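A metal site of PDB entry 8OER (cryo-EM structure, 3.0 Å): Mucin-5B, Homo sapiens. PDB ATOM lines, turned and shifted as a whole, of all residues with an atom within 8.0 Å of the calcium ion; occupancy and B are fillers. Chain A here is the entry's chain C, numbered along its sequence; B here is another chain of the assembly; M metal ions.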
ATOM      1  N   THR A 113       8.446  14.814 -35.241  1.00  0.00           N
ATOM      2  CA  THR A 113       8.104  14.028 -34.064  1.00  0.00           C
ATOM      3  C   THR A 113       6.764  13.328 -34.255  1.00  0.00           C
ATOM      4  O   THR A 113       6.134  13.390 -35.313  1.00  0.00           O
ATOM      5  CB  THR A 113       8.063  14.906 -32.833  1.00  0.00           C
ATOM      6  OG1 THR A 113       7.209  14.292 -31.866  1.00  0.00           O
ATOM      7  CG2 THR A 113       7.540  16.256 -33.162  1.00  0.00           C
ATOM      8  N   PHE A 114       6.347  12.637 -33.197  1.00  0.00           N
ATOM      9  CA  PHE A 114       5.128  11.837 -33.260  1.00  0.00           C
ATOM     10  C   PHE A 114       3.907  12.714 -33.482  1.00  0.00           C
ATOM     11  O   PHE A 114       3.006  12.353 -34.247  1.00  0.00           O
ATOM     12  CB  PHE A 114       4.969  11.044 -31.970  1.00  0.00           C
ATOM     13  CG  PHE A 114       5.801   9.788 -31.901  1.00  0.00           C
ATOM     14  CD1 PHE A 114       5.512   8.714 -32.722  1.00  0.00           C
ATOM     15  CD2 PHE A 114       6.830   9.675 -31.000  1.00  0.00           C
ATOM     16  CE1 PHE A 114       6.265   7.566 -32.637  1.00  0.00           C
ATOM     17  CE2 PHE A 114       7.574   8.524 -30.926  1.00  0.00           C
ATOM     18  CZ  PHE A 114       7.299   7.475 -31.737  1.00  0.00           C
ATOM     19  N   ASP A 115       3.850  13.862 -32.814  1.00  0.00           N
ATOM     20  CA  ASP A 115       2.722  14.779 -32.888  1.00  0.00           C
ATOM     21  C   ASP A 115       2.713  15.625 -34.141  1.00  0.00           C
ATOM     22  O   ASP A 115       1.942  16.586 -34.209  1.00  0.00           O
ATOM     23  CB  ASP A 115       2.704  15.697 -31.672  1.00  0.00           C
ATOM     24  CG  ASP A 115       2.534  14.943 -30.375  1.00  0.00           C
ATOM     25  OD1 ASP A 115       1.662  14.055 -30.311  1.00  0.00           O
ATOM     26  OD2 ASP A 115       3.294  15.223 -29.437  1.00  0.00           O
ATOM     27  N   ASP A 117       5.019  17.685 -35.337  1.00  0.00           N
ATOM     28  CA  ASP A 117       5.886  18.854 -35.380  1.00  0.00           C
ATOM     29  C   ASP A 117       7.148  18.557 -36.175  1.00  0.00           C
ATOM     30  O   ASP A 117       7.614  17.426 -36.238  1.00  0.00           O
ATOM     31  CB  ASP A 117       6.249  19.306 -33.965  1.00  0.00           C
ATOM     32  CG  ASP A 117       6.936  20.642 -33.939  1.00  0.00           C
ATOM     33  OD1 ASP A 117       7.071  21.264 -35.015  1.00  0.00           O
ATOM     34  OD2 ASP A 117       7.350  21.080 -32.858  1.00  0.00           O
ATOM     35  N   GLY A 228       1.410   9.523 -24.989  1.00  0.00           N
ATOM     36  CA  GLY A 228       1.570  10.398 -23.850  1.00  0.00           C
ATOM     37  C   GLY A 228       2.612   9.991 -22.846  1.00  0.00           C
ATOM     38  O   GLY A 228       2.894  10.767 -21.913  1.00  0.00           O
ATOM     39  N   CYS A 234      11.494  12.662 -30.176  1.00  0.00           N
ATOM     40  CA  CYS A 234      10.251  12.434 -30.901  1.00  0.00           C
ATOM     41  C   CYS A 234       9.056  12.950 -30.120  1.00  0.00           C
ATOM     42  O   CYS A 234       7.944  12.417 -30.258  1.00  0.00           O
ATOM     43  CB  CYS A 234      10.084  10.952 -31.230  1.00  0.00           C
ATOM     44  SG  CYS A 234      11.356  10.260 -32.298  1.00  0.00           S
ATOM     45  N   GLY A 235       9.251  13.961 -29.282  1.00  0.00           N
ATOM     46  CA  GLY A 235       8.163  14.530 -28.546  1.00  0.00           C
ATOM     47  C   GLY A 235       7.667  13.553 -27.500  1.00  0.00           C
ATOM     48  O   GLY A 235       8.303  12.545 -27.199  1.00  0.00           O
ATOM     49  N   ASN A 236       6.505  13.862 -26.955  1.00  0.00           N
ATOM     50  CA  ASN A 236       5.883  13.016 -25.956  1.00  0.00           C
ATOM     51  C   ASN A 236       4.629  12.323 -26.462  1.00  0.00           C
ATOM     52  O   ASN A 236       3.902  11.725 -25.664  1.00  0.00           O
ATOM     53  CB  ASN A 236       5.573  13.812 -24.693  1.00  0.00           C
ATOM     54  CG  ASN A 236       4.448  14.791 -24.877  1.00  0.00           C
ATOM     55  OD1 ASN A 236       4.266  15.357 -25.953  1.00  0.00           O
ATOM     56  ND2 ASN A 236       3.684  15.013 -23.821  1.00  0.00           N
ATOM     57  N   PHE A 237       4.354  12.389 -27.762  1.00  0.00           N
ATOM     58  CA  PHE A 237       3.257  11.646 -28.365  1.00  0.00           C
ATOM     59  C   PHE A 237       1.952  11.902 -27.625  1.00  0.00           C
ATOM     60  O   PHE A 237       1.345  11.008 -27.044  1.00  0.00           O
ATOM     61  CB  PHE A 237       3.581  10.152 -28.397  1.00  0.00           C
ATOM     62  CG  PHE A 237       2.683   9.345 -29.285  1.00  0.00           C
ATOM     63  CD1 PHE A 237       1.819   9.956 -30.163  1.00  0.00           C
ATOM     64  CD2 PHE A 237       2.715   7.967 -29.240  1.00  0.00           C
ATOM     65  CE1 PHE A 237       1.007   9.195 -30.976  1.00  0.00           C
ATOM     66  CE2 PHE A 237       1.907   7.215 -30.050  1.00  0.00           C
ATOM     67  CZ  PHE A 237       1.045   7.831 -30.912  1.00  0.00           C
ATOM     68  N   ASP A 238       1.515  13.161 -27.630  1.00  0.00           N
ATOM     69  CA  ASP A 238       0.321  13.555 -26.908  1.00  0.00           C
ATOM     70  C   ASP A 238      -0.720  14.208 -27.806  1.00  0.00           C
ATOM     71  O   ASP A 238      -1.731  14.710 -27.294  1.00  0.00           O
ATOM     72  CB  ASP A 238       0.668  14.489 -25.751  1.00  0.00           C
ATOM     73  CG  ASP A 238       1.369  15.755 -26.215  1.00  0.00           C
ATOM     74  OD1 ASP A 238       1.800  15.808 -27.373  1.00  0.00           O
ATOM     75  OD2 ASP A 238       1.478  16.708 -25.417  1.00  0.00           O
ATOM     76  N   ASP A 239      -0.514  14.201 -29.124  1.00  0.00           N
ATOM     77  CA  ASP A 239      -1.373  14.927 -30.063  1.00  0.00           C
ATOM     78  C   ASP A 239      -1.463  16.394 -29.675  1.00  0.00           C
ATOM     79  O   ASP A 239      -2.524  17.016 -29.723  1.00  0.00           O
ATOM     80  CB  ASP A 239      -2.757  14.309 -30.155  1.00  0.00           C
ATOM     81  CG  ASP A 239      -2.713  12.803 -30.235  1.00  0.00           C
ATOM     82  OD1 ASP A 239      -2.145  12.180 -29.312  1.00  0.00           O
ATOM     83  OD2 ASP A 239      -3.247  12.239 -31.216  1.00  0.00           O
ATOM     84  N   ASN A 240      -0.334  16.965 -29.270  1.00  0.00           N
ATOM     85  CA  ASN A 240      -0.239  18.381 -28.914  1.00  0.00           C
ATOM     86  C   ASN A 240       1.169  18.816 -29.314  1.00  0.00           C
ATOM     87  O   ASN A 240       2.112  18.677 -28.543  1.00  0.00           O
ATOM     88  CB  ASN A 240      -0.496  18.594 -27.431  1.00  0.00           C
ATOM     89  CG  ASN A 240      -0.388  20.056 -27.023  1.00  0.00           C
ATOM     90  OD1 ASN A 240       0.028  20.899 -27.807  1.00  0.00           O
ATOM     91  ND2 ASN A 240      -0.753  20.345 -25.790  1.00  0.00           N
ATOM     92  N   ALA A 241       1.286  19.344 -30.529  1.00  0.00           N
ATOM     93  CA  ALA A 241       2.592  19.583 -31.126  1.00  0.00           C
ATOM     94  C   ALA A 241       3.232  20.870 -30.661  1.00  0.00           C
ATOM     95  O   ALA A 241       4.427  21.064 -30.899  1.00  0.00           O
ATOM     96  CB  ALA A 241       2.468  19.598 -32.643  1.00  0.00           C
ATOM     97  N   ILE A 242       2.482  21.765 -30.011  1.00  0.00           N
ATOM     98  CA  ILE A 242       3.067  23.032 -29.607  1.00  0.00           C
ATOM     99  C   ILE A 242       4.052  22.818 -28.458  1.00  0.00           C
ATOM    100  O   ILE A 242       5.096  23.464 -28.403  1.00  0.00           O
ATOM    101  CB  ILE A 242       1.956  24.029 -29.234  1.00  0.00           C
ATOM    102  CG1 ILE A 242       0.678  23.732 -30.013  1.00  0.00           C
ATOM    103  CG2 ILE A 242       2.428  25.446 -29.509  1.00  0.00           C
ATOM    104  CD1 ILE A 242      -0.508  24.560 -29.585  1.00  0.00           C
ATOM    105  N   ASN A 243       3.726  21.924 -27.533  1.00  0.00           N
ATOM    106  CA  ASN A 243       4.530  21.698 -26.344  1.00  0.00           C
ATOM    107  C   ASN A 243       5.519  20.545 -26.499  1.00  0.00           C
ATOM    108  O   ASN A 243       6.142  20.142 -25.511  1.00  0.00           O
ATOM    109  CB  ASN A 243       3.634  21.447 -25.134  1.00  0.00           C
ATOM    110  CG  ASN A 243       3.358  19.980 -24.910  1.00  0.00           C
ATOM    111  OD1 ASN A 243       2.996  19.253 -25.826  1.00  0.00           O
ATOM    112  ND2 ASN A 243       3.551  19.529 -23.676  1.00  0.00           N
ATOM    113  N   ASP A 244       5.686  20.021 -27.713  1.00  0.00           N
ATOM    114  CA  ASP A 244       6.627  18.921 -27.910  1.00  0.00           C
ATOM    115  C   ASP A 244       8.072  19.346 -27.703  1.00  0.00           C
ATOM    116  O   ASP A 244       8.938  18.467 -27.640  1.00  0.00           O
ATOM    117  CB  ASP A 244       6.478  18.332 -29.297  1.00  0.00           C
ATOM    118  CG  ASP A 244       5.833  16.977 -29.266  1.00  0.00           C
ATOM    119  OD1 ASP A 244       5.235  16.654 -28.232  1.00  0.00           O
ATOM    120  OD2 ASP A 244       5.931  16.247 -30.263  1.00  0.00           O
ATOM    121  N   PHE A 245       8.354  20.638 -27.612  1.00  0.00           N
ATOM    122  CA  PHE A 245       9.686  21.075 -27.240  1.00  0.00           C
ATOM    123  C   PHE A 245       9.842  21.058 -25.731  1.00  0.00           C
ATOM    124  O   PHE A 245      10.217  22.067 -25.123  1.00  0.00           O
ATOM    125  CB  PHE A 245       9.953  22.481 -27.778  1.00  0.00           C
ATOM    126  CG  PHE A 245      10.412  22.506 -29.197  1.00  0.00           C
ATOM    127  CD1 PHE A 245      10.116  21.472 -30.055  1.00  0.00           C
ATOM    128  CD2 PHE A 245      11.159  23.560 -29.673  1.00  0.00           C
ATOM    129  CE1 PHE A 245      10.542  21.496 -31.355  1.00  0.00           C
ATOM    130  CE2 PHE A 245      11.589  23.592 -30.970  1.00  0.00           C
ATOM    131  CZ  PHE A 245      11.278  22.563 -31.814  1.00  0.00           C
ATOM    132  N   ALA A 246       9.538  19.928 -25.112  1.00  0.00           N
ATOM    133  CA  ALA A 246       9.620  19.771 -23.668  1.00  0.00           C
ATOM    134  C   ALA A 246      10.960  19.139 -23.309  1.00  0.00           C
ATOM    135  O   ALA A 246      11.225  17.985 -23.673  1.00  0.00           O
ATOM    136  CB  ALA A 246       8.475  18.912 -23.142  1.00  0.00           C
ATOM    137  N   VAL A 252       8.805  23.774 -21.431  1.00  0.00           N
ATOM    138  CA  VAL A 252       8.592  23.889 -22.861  1.00  0.00           C
ATOM    139  C   VAL A 252       9.232  25.168 -23.372  1.00  0.00           C
ATOM    140  O   VAL A 252       8.950  26.264 -22.885  1.00  0.00           O
ATOM    141  CB  VAL A 252       7.097  23.846 -23.195  1.00  0.00           C
ATOM    142  CG1 VAL A 252       6.858  24.411 -24.581  1.00  0.00           C
ATOM    143  CG2 VAL A 252       6.584  22.432 -23.098  1.00  0.00           C
ATOM    144  N   GLN B 542      -5.566  22.397 -29.432  1.00  0.00           N
ATOM    145  CA  GLN B 542      -4.183  22.051 -29.106  1.00  0.00           C
ATOM    146  C   GLN B 542      -3.768  20.733 -29.767  1.00  0.00           C
ATOM    147  O   GLN B 542      -3.395  19.754 -29.121  1.00  0.00           O
ATOM    148  CB  GLN B 542      -3.991  22.013 -27.594  1.00  0.00           C
ATOM    149  CG  GLN B 542      -4.628  23.164 -26.865  1.00  0.00           C
ATOM    150  CD  GLN B 542      -4.357  24.490 -27.518  1.00  0.00           C
ATOM    151  OE1 GLN B 542      -3.266  24.735 -28.041  1.00  0.00           O
ATOM    152  NE2 GLN B 542      -5.341  25.375 -27.486  1.00  0.00           N
HETATM  153 CA    CA M   1       3.300  17.328 -27.052  1.00  0.00          CA
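The side-chain carboxylate (OD1) of Asp 115 is in hydrogen-bond range of the backbone NH (N) of Asp 238.
The side-chain amide oxygen (OD1) of Asn 240 lies close to the backbone NH (N) of Ile 242 (3.4 Å).
The side-chain carboxylate of Asp 244 sits close to the side-chain carboxylate of Asp 115.
OD2 of Asp 244 sits at hydrogen-bond distance from OG1 of Thr 113, 2.8 Å away.
The backbone carbonyl oxygen of Asn 236 lies close to the backbone NH of Gly 228, 3.4 Å away.
The side-chain carboxylate (OD2) of Asp 115 sits at hydrogen-bond distance from the backbone NH (N) of Phe 237, 3.5 Å away.
The backbone NH (N) of Asp 239 is in hydrogen-bond range of the side-chain carboxylate (OD1) of Asp 115.
The calcium ion is bound by OD1 of Asp 238, OD1 of Asn 243, O of Asn 240, OD1 of Asp 244, OD1 of Asn 236 and OD2 of Asp 238.
The calcium ion has six donor atoms within binding distance.
Asp 115 touches the calcium ion.
Within 4 Å of the calcium ion: Asp 115, Asn 236, Asp 238, Asn 240, Asn 243 and Asp 244.
The nearest printed residue that does not touch the calcium ion is Ala 241 (4.5 Å).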
